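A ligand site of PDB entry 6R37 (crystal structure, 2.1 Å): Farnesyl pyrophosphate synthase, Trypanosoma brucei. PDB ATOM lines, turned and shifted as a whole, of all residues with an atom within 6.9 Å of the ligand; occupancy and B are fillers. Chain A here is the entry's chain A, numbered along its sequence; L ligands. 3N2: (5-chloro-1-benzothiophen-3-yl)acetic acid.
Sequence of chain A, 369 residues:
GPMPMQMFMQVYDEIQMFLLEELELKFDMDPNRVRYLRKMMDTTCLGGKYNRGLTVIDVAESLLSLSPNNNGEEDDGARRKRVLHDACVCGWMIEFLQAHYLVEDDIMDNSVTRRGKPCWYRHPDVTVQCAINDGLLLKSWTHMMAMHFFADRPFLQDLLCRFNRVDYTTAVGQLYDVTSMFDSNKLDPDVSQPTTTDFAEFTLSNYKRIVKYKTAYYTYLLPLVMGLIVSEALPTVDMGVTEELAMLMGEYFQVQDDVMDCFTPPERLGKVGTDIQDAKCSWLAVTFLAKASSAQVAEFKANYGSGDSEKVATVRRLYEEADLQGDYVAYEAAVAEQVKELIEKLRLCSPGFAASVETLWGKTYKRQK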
ATOM      1  N   GLY A  48      17.003 -10.123  19.780  1.00  0.00           N
ATOM      2  CA  GLY A  48      18.301 -10.047  20.441  1.00  0.00           C
ATOM      3  C   GLY A  48      19.351  -9.376  19.573  1.00  0.00           C
ATOM      4  O   GLY A  48      19.027  -8.743  18.565  1.00  0.00           O
ATOM      5  N   LYS A  49      20.645  -9.497  19.957  1.00  0.00           N
ATOM      6  CA  LYS A  49      21.713  -8.887  19.167  1.00  0.00           C
ATOM      7  C   LYS A  49      22.299  -9.877  18.153  1.00  0.00           C
ATOM      8  O   LYS A  49      22.993  -9.462  17.216  1.00  0.00           O
ATOM      9  CB  LYS A  49      22.810  -8.287  20.075  1.00  0.00           C
ATOM     10  CG  LYS A  49      23.544  -7.107  19.414  1.00  0.00           C
ATOM     11  CD  LYS A  49      24.694  -6.593  20.275  1.00  0.00           C
ATOM     12  CE  LYS A  49      25.431  -5.452  19.626  1.00  0.00           C
ATOM     13  NZ  LYS A  49      26.653  -5.074  20.372  1.00  0.00           N
ATOM     14  N   TYR A  50      22.005 -11.177  18.332  1.00  0.00           N
ATOM     15  CA  TYR A  50      22.450 -12.305  17.529  1.00  0.00           C
ATOM     16  C   TYR A  50      23.968 -12.486  17.576  1.00  0.00           C
ATOM     17  O   TYR A  50      24.572 -12.939  16.607  1.00  0.00           O
ATOM     18  CB  TYR A  50      21.911 -12.239  16.086  1.00  0.00           C
ATOM     19  CG  TYR A  50      20.433 -11.871  15.987  1.00  0.00           C
ATOM     20  CD1 TYR A  50      19.445 -12.777  16.370  1.00  0.00           C
ATOM     21  CD2 TYR A  50      20.025 -10.618  15.540  1.00  0.00           C
ATOM     22  CE1 TYR A  50      18.093 -12.455  16.284  1.00  0.00           C
ATOM     23  CE2 TYR A  50      18.674 -10.288  15.450  1.00  0.00           C
ATOM     24  CZ  TYR A  50      17.710 -11.213  15.821  1.00  0.00           C
ATOM     25  OH  TYR A  50      16.366 -10.889  15.740  1.00  0.00           O
ATOM     26  N   ASN A  51      24.575 -12.127  18.720  1.00  0.00           N
ATOM     27  CA  ASN A  51      26.026 -12.214  18.912  1.00  0.00           C
ATOM     28  C   ASN A  51      26.565 -13.623  18.671  1.00  0.00           C
ATOM     29  O   ASN A  51      27.569 -13.760  17.968  1.00  0.00           O
ATOM     30  CB  ASN A  51      26.460 -11.668  20.272  1.00  0.00           C
ATOM     31  CG  ASN A  51      26.333 -10.178  20.436  1.00  0.00           C
ATOM     32  OD1 ASN A  51      26.750  -9.399  19.570  1.00  0.00           O
ATOM     33  ND2 ASN A  51      25.763  -9.747  21.557  1.00  0.00           N
ATOM     34  N   ARG A  52      25.886 -14.670  19.183  1.00  0.00           N
ATOM     35  CA  ARG A  52      26.318 -16.059  18.988  1.00  0.00           C
ATOM     36  C   ARG A  52      26.196 -16.480  17.516  1.00  0.00           C
ATOM     37  O   ARG A  52      27.145 -17.058  16.962  1.00  0.00           O
ATOM     38  CB  ARG A  52      25.546 -17.045  19.895  1.00  0.00           C
ATOM     39  CG  ARG A  52      25.873 -16.925  21.384  1.00  0.00           C
ATOM     40  CD  ARG A  52      24.819 -17.646  22.221  1.00  0.00           C
ATOM     41  NE  ARG A  52      24.939 -17.350  23.653  1.00  0.00           N
ATOM     42  CZ  ARG A  52      24.450 -16.263  24.251  1.00  0.00           C
ATOM     43  NH1 ARG A  52      23.830 -15.331  23.548  1.00  0.00           N
ATOM     44  NH2 ARG A  52      24.590 -16.105  25.557  1.00  0.00           N
ATOM     45  N   GLY A  53      25.045 -16.185  16.903  1.00  0.00           N
ATOM     46  CA  GLY A  53      24.733 -16.502  15.516  1.00  0.00           C
ATOM     47  C   GLY A  53      25.617 -15.802  14.515  1.00  0.00           C
ATOM     48  O   GLY A  53      26.169 -16.433  13.611  1.00  0.00           O
ATOM     49  N   THR A  55      28.579 -14.582  15.097  1.00  0.00           N
ATOM     50  CA  THR A  55      29.954 -15.061  15.294  1.00  0.00           C
ATOM     51  C   THR A  55      30.251 -16.210  14.331  1.00  0.00           C
ATOM     52  O   THR A  55      31.349 -16.247  13.782  1.00  0.00           O
ATOM     53  CB  THR A  55      30.226 -15.430  16.778  1.00  0.00           C
ATOM     54  OG1 THR A  55      30.097 -14.255  17.576  1.00  0.00           O
ATOM     55  CG2 THR A  55      31.630 -15.996  17.007  1.00  0.00           C
ATOM     56  N   GLU A  95      21.159 -19.701  18.197  1.00  0.00           N
ATOM     57  CA  GLU A  95      20.141 -18.719  18.584  1.00  0.00           C
ATOM     58  C   GLU A  95      18.875 -19.434  19.098  1.00  0.00           C
ATOM     59  O   GLU A  95      18.310 -19.004  20.112  1.00  0.00           O
ATOM     60  CB  GLU A  95      19.828 -17.747  17.425  1.00  0.00           C
ATOM     61  CG  GLU A  95      20.933 -16.755  17.109  1.00  0.00           C
ATOM     62  CD  GLU A  95      21.446 -15.869  18.246  1.00  0.00           C
ATOM     63  OE1 GLU A  95      22.683 -15.673  18.326  1.00  0.00           O
ATOM     64  OE2 GLU A  95      20.622 -15.379  19.049  1.00  0.00           O
ATOM     65  N   GLN A  98      19.741 -20.897  22.552  1.00  0.00           N
ATOM     66  CA  GLN A  98      19.661 -19.766  23.485  1.00  0.00           C
ATOM     67  C   GLN A  98      18.191 -19.489  23.825  1.00  0.00           C
ATOM     68  O   GLN A  98      17.847 -19.413  25.011  1.00  0.00           O
ATOM     69  CB  GLN A  98      20.365 -18.519  22.902  1.00  0.00           C
ATOM     70  CG  GLN A  98      20.183 -17.165  23.665  1.00  0.00           C
ATOM     71  CD  GLN A  98      20.698 -17.121  25.079  1.00  0.00           C
ATOM     72  OE1 GLN A  98      21.111 -18.119  25.659  1.00  0.00           O
ATOM     73  NE2 GLN A  98      20.685 -15.952  25.691  1.00  0.00           N
ATOM     74  N   TYR A 218      28.837 -22.665  25.350  1.00  0.00           N
ATOM     75  CA  TYR A 218      27.801 -22.424  24.339  1.00  0.00           C
ATOM     76  C   TYR A 218      27.822 -20.993  23.743  1.00  0.00           C
ATOM     77  O   TYR A 218      27.473 -20.834  22.576  1.00  0.00           O
ATOM     78  CB  TYR A 218      26.375 -22.831  24.854  1.00  0.00           C
ATOM     79  CG  TYR A 218      25.530 -21.721  25.453  1.00  0.00           C
ATOM     80  CD1 TYR A 218      25.629 -21.388  26.805  1.00  0.00           C
ATOM     81  CD2 TYR A 218      24.575 -21.045  24.683  1.00  0.00           C
ATOM     82  CE1 TYR A 218      24.826 -20.401  27.371  1.00  0.00           C
ATOM     83  CE2 TYR A 218      23.773 -20.041  25.239  1.00  0.00           C
ATOM     84  CZ  TYR A 218      23.896 -19.727  26.579  1.00  0.00           C
ATOM     85  OH  TYR A 218      23.130 -18.733  27.141  1.00  0.00           O
ATOM     86  N   THR A 219      28.237 -19.991  24.538  1.00  0.00           N
ATOM     87  CA  THR A 219      28.285 -18.596  24.110  1.00  0.00           C
ATOM     88  C   THR A 219      29.546 -18.258  23.325  1.00  0.00           C
ATOM     89  O   THR A 219      29.450 -17.545  22.321  1.00  0.00           O
ATOM     90  CB  THR A 219      28.093 -17.681  25.322  1.00  0.00           C
ATOM     91  OG1 THR A 219      26.871 -18.046  25.958  1.00  0.00           O
ATOM     92  CG2 THR A 219      28.040 -16.199  24.960  1.00  0.00           C
ATOM     93  N   TYR A 220      30.736 -18.732  23.781  1.00  0.00           N
ATOM     94  CA  TYR A 220      32.002 -18.392  23.125  1.00  0.00           C
ATOM     95  C   TYR A 220      32.616 -19.529  22.346  1.00  0.00           C
ATOM     96  O   TYR A 220      33.019 -19.293  21.217  1.00  0.00           O
ATOM     97  CB  TYR A 220      33.010 -17.796  24.120  1.00  0.00           C
ATOM     98  CG  TYR A 220      32.548 -16.458  24.659  1.00  0.00           C
ATOM     99  CD1 TYR A 220      32.896 -15.268  24.013  1.00  0.00           C
ATOM    100  CD2 TYR A 220      31.685 -16.381  25.747  1.00  0.00           C
ATOM    101  CE1 TYR A 220      32.412 -14.045  24.464  1.00  0.00           C
ATOM    102  CE2 TYR A 220      31.210 -15.164  26.207  1.00  0.00           C
ATOM    103  CZ  TYR A 220      31.568 -13.992  25.552  1.00  0.00           C
ATOM    104  OH  TYR A 220      31.096 -12.777  25.988  1.00  0.00           O
ATOM    105  N   PRO A 223      30.046 -21.099  18.999  1.00  0.00           N
ATOM    106  CA  PRO A 223      30.005 -20.340  17.730  1.00  0.00           C
ATOM    107  C   PRO A 223      31.300 -20.419  16.939  1.00  0.00           C
ATOM    108  O   PRO A 223      31.251 -20.597  15.731  1.00  0.00           O
ATOM    109  CB  PRO A 223      29.664 -18.905  18.167  1.00  0.00           C
ATOM    110  CG  PRO A 223      29.051 -19.052  19.499  1.00  0.00           C
ATOM    111  CD  PRO A 223      29.746 -20.205  20.140  1.00  0.00           C
ATOM    112  N   PHE A 253      33.219 -11.525  30.396  1.00  0.00           N
ATOM    113  CA  PHE A 253      31.818 -11.188  30.207  1.00  0.00           C
ATOM    114  C   PHE A 253      30.992 -11.400  31.481  1.00  0.00           C
ATOM    115  O   PHE A 253      30.154 -10.550  31.793  1.00  0.00           O
ATOM    116  CB  PHE A 253      31.262 -12.032  29.040  1.00  0.00           C
ATOM    117  CG  PHE A 253      29.769 -12.094  28.905  1.00  0.00           C
ATOM    118  CD1 PHE A 253      29.061 -11.033  28.365  1.00  0.00           C
ATOM    119  CD2 PHE A 253      29.067 -13.220  29.333  1.00  0.00           C
ATOM    120  CE1 PHE A 253      27.679 -11.068  28.271  1.00  0.00           C
ATOM    121  CE2 PHE A 253      27.679 -13.268  29.216  1.00  0.00           C
ATOM    122  CZ  PHE A 253      26.988 -12.194  28.681  1.00  0.00           C
ATOM    123  N   GLN A 256      31.760  -8.813  34.357  1.00  0.00           N
ATOM    124  CA  GLN A 256      31.117  -7.564  33.980  1.00  0.00           C
ATOM    125  C   GLN A 256      29.608  -7.679  34.186  1.00  0.00           C
ATOM    126  O   GLN A 256      29.007  -6.743  34.702  1.00  0.00           O
ATOM    127  CB  GLN A 256      31.446  -7.214  32.529  1.00  0.00           C
ATOM    128  CG  GLN A 256      30.785  -5.930  32.048  1.00  0.00           C
ATOM    129  CD  GLN A 256      31.275  -5.512  30.696  1.00  0.00           C
ATOM    130  OE1 GLN A 256      31.308  -6.288  29.739  1.00  0.00           O
ATOM    131  NE2 GLN A 256      31.646  -4.257  30.590  1.00  0.00           N
ATOM    132  N   ASP A 257      29.013  -8.838  33.793  1.00  0.00           N
ATOM    133  CA  ASP A 257      27.583  -9.095  33.935  1.00  0.00           C
ATOM    134  C   ASP A 257      27.156  -9.079  35.400  1.00  0.00           C
ATOM    135  O   ASP A 257      26.114  -8.518  35.723  1.00  0.00           O
ATOM    136  CB  ASP A 257      27.219 -10.451  33.293  1.00  0.00           C
ATOM    137  CG  ASP A 257      25.865 -10.508  32.619  1.00  0.00           C
ATOM    138  OD1 ASP A 257      25.550  -9.582  31.835  1.00  0.00           O
ATOM    139  OD2 ASP A 257      25.130 -11.503  32.846  1.00  0.00           O
ATOM    140  N   LEU A 360      35.081 -11.014  17.949  1.00  0.00           N
ATOM    141  CA  LEU A 360      34.272 -11.612  19.018  1.00  0.00           C
ATOM    142  C   LEU A 360      34.649 -10.976  20.350  1.00  0.00           C
ATOM    143  O   LEU A 360      33.761 -10.579  21.102  1.00  0.00           O
ATOM    144  CB  LEU A 360      34.379 -13.156  19.066  1.00  0.00           C
ATOM    145  CG  LEU A 360      33.649 -13.911  20.234  1.00  0.00           C
ATOM    146  CD1 LEU A 360      32.149 -13.655  20.240  1.00  0.00           C
ATOM    147  CD2 LEU A 360      33.908 -15.393  20.183  1.00  0.00           C
ATOM    148  N   TRP A 361      35.958 -10.806  20.599  1.00  0.00           N
ATOM    149  CA  TRP A 361      36.495 -10.157  21.784  1.00  0.00           C
ATOM    150  C   TRP A 361      36.069  -8.689  21.895  1.00  0.00           C
ATOM    151  O   TRP A 361      35.651  -8.260  22.967  1.00  0.00           O
ATOM    152  CB  TRP A 361      38.015 -10.321  21.822  1.00  0.00           C
ATOM    153  CG  TRP A 361      38.707  -9.521  22.883  1.00  0.00           C
ATOM    154  CD1 TRP A 361      39.714  -8.626  22.691  1.00  0.00           C
ATOM    155  CD2 TRP A 361      38.452  -9.558  24.290  1.00  0.00           C
ATOM    156  NE1 TRP A 361      40.101  -8.102  23.901  1.00  0.00           N
ATOM    157  CE2 TRP A 361      39.347  -8.652  24.900  1.00  0.00           C
ATOM    158  CE3 TRP A 361      37.567 -10.278  25.106  1.00  0.00           C
ATOM    159  CZ2 TRP A 361      39.394  -8.459  26.280  1.00  0.00           C
ATOM    160  CZ3 TRP A 361      37.594 -10.068  26.474  1.00  0.00           C
ATOM    161  CH2 TRP A 361      38.503  -9.173  27.045  1.00  0.00           C
ATOM    162  N   GLY A 362      36.142  -7.945  20.780  1.00  0.00           N
ATOM    163  CA  GLY A 362      35.700  -6.559  20.719  1.00  0.00           C
ATOM    164  C   GLY A 362      34.241  -6.383  21.126  1.00  0.00           C
ATOM    165  O   GLY A 362      33.906  -5.412  21.801  1.00  0.00           O
ATOM    166  N   LYS A 363      33.365  -7.366  20.774  1.00  0.00           N
ATOM    167  CA  LYS A 363      31.954  -7.373  21.146  1.00  0.00           C
ATOM    168  C   LYS A 363      31.757  -7.532  22.671  1.00  0.00           C
ATOM    169  O   LYS A 363      30.784  -6.998  23.204  1.00  0.00           O
ATOM    170  CB  LYS A 363      31.191  -8.479  20.394  1.00  0.00           C
ATOM    171  CG  LYS A 363      31.100  -8.244  18.893  1.00  0.00           C
ATOM    172  CD  LYS A 363      30.226  -9.283  18.211  1.00  0.00           C
ATOM    173  CE  LYS A 363      30.932  -9.929  17.045  1.00  0.00           C
ATOM    174  NZ  LYS A 363      30.335  -9.505  15.750  1.00  0.00           N
ATOM    175  N   THR A 364      32.684  -8.247  23.345  1.00  0.00           N
ATOM    176  CA  THR A 364      32.707  -8.498  24.788  1.00  0.00           C
ATOM    177  C   THR A 364      33.353  -7.327  25.564  1.00  0.00           C
ATOM    178  O   THR A 364      32.812  -6.888  26.576  1.00  0.00           O
ATOM    179  CB  THR A 364      33.470  -9.804  25.096  1.00  0.00           C
ATOM    180  OG1 THR A 364      32.978 -10.853  24.270  1.00  0.00           O
ATOM    181  CG2 THR A 364      33.411 -10.198  26.560  1.00  0.00           C
ATOM    182  N   TYR A 365      34.519  -6.858  25.090  1.00  0.00           N
ATOM    183  CA  TYR A 365      35.313  -5.782  25.688  1.00  0.00           C
ATOM    184  C   TYR A 365      34.565  -4.414  25.663  1.00  0.00           C
ATOM    185  O   TYR A 365      34.820  -3.593  26.524  1.00  0.00           O
ATOM    186  CB  TYR A 365      36.688  -5.737  25.026  1.00  0.00           C
ATOM    187  CG  TYR A 365      37.705  -4.849  25.700  1.00  0.00           C
ATOM    188  CD1 TYR A 365      38.052  -3.608  25.149  1.00  0.00           C
ATOM    189  CD2 TYR A 365      38.382  -5.269  26.844  1.00  0.00           C
ATOM    190  CE1 TYR A 365      39.037  -2.809  25.739  1.00  0.00           C
ATOM    191  CE2 TYR A 365      39.355  -4.463  27.448  1.00  0.00           C
ATOM    192  CZ  TYR A 365      39.677  -3.237  26.887  1.00  0.00           C
ATOM    193  OH  TYR A 365      40.612  -2.435  27.478  1.00  0.00           O
ATOM    194  N   LYS A 366      33.580  -4.253  24.741  1.00  0.00           N
ATOM    195  CA  LYS A 366      32.711  -3.065  24.560  1.00  0.00           C
ATOM    196  C   LYS A 366      31.779  -2.846  25.776  1.00  0.00           C
ATOM    197  O   LYS A 366      30.551  -2.913  25.682  1.00  0.00           O
ATOM    198  CB  LYS A 366      31.894  -3.216  23.254  1.00  0.00           C
ATOM    199  CG  LYS A 366      31.410  -1.915  22.634  1.00  0.00           C
ATOM    200  CD  LYS A 366      31.190  -2.084  21.132  1.00  0.00           C
ATOM    201  CE  LYS A 366      30.372  -0.970  20.531  1.00  0.00           C
ATOM    202  NZ  LYS A 366      28.914  -1.205  20.708  1.00  0.00           N
HETATM  203 CL1  3N2 L   1      28.906 -14.405  22.033  1.00  0.00          CL
HETATM  204  C2  3N2 L   1      28.709 -12.849  22.790  1.00  0.00           C
HETATM  205  C3  3N2 L   1      27.589 -12.613  23.597  1.00  0.00           C
HETATM  206  C5  3N2 L   1      27.446 -11.339  24.157  1.00  0.00           C
HETATM  207  C6  3N2 L   1      28.369 -10.322  23.909  1.00  0.00           C
HETATM  208  S7  3N2 L   1      28.029  -8.779  24.688  1.00  0.00           S
HETATM  209  C8  3N2 L   1      26.574  -9.493  25.349  1.00  0.00           C
HETATM  210  C10 3N2 L   1      26.348 -10.778  25.039  1.00  0.00           C
HETATM  211  C11 3N2 L   1      25.193 -11.591  25.572  1.00  0.00           C
HETATM  212  C14 3N2 L   1      24.196 -12.078  24.550  1.00  0.00           C
HETATM  213  O15 3N2 L   1      24.438 -11.754  23.270  1.00  0.00           O
HETATM  214  O16 3N2 L   1      23.217 -12.728  24.900  1.00  0.00           O
HETATM  215  C18 3N2 L   1      29.489 -10.549  23.098  1.00  0.00           C
HETATM  216  C20 3N2 L   1      29.651 -11.829  22.528  1.00  0.00           C
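ND2 of Asn 51 is in hydrogen-bond range of O15 of the ligand.
The guanidinium group of Arg 52 lies within salt-bridge range of an oxygen (O16) of the ligand, at 3.0 Å.
O of Lys 363 sits close to S7 of the ligand, at 3.6 Å.
Merely in contact with the ligand: Thr 219 (3.2 Å), Tyr 220 (3.9 Å), Phe 253 (3.5 Å), Leu 360 (3.8 Å) and Thr 364 (3.7 Å).
Hydrophobic or aromatic side chains within 4 Å of the ligand: Phe 253 and Leu 360.
Of the 23 residues printed, 8 come within 4 Å of the ligand.
The side-chain hydroxyl (OG1) of Thr 55 lies within hydrogen-bond range of the backbone carbonyl oxygen (O) of Asn 51 (2.6 Å).
The guanidinium group of Arg 52 is in hydrogen-bond range of the side-chain hydroxyl of Thr 219 (3.0 Å).
The guanidinium group (NH2) of Arg 52 is in hydrogen-bond range of the side-chain hydroxyl (OH) of Tyr 218 (3.4 Å).
N of Arg 52 lies within hydrogen-bond range of OE1 of Glu 95 (3.5 Å).
The side-chain hydroxyl of Thr 364 is in hydrogen-bond range of the backbone carbonyl oxygen of Leu 360, 3.3 Å away.
OG1 of Thr 364 is in hydrogen-bond range of OH of Tyr 220, 3.2 Å away.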
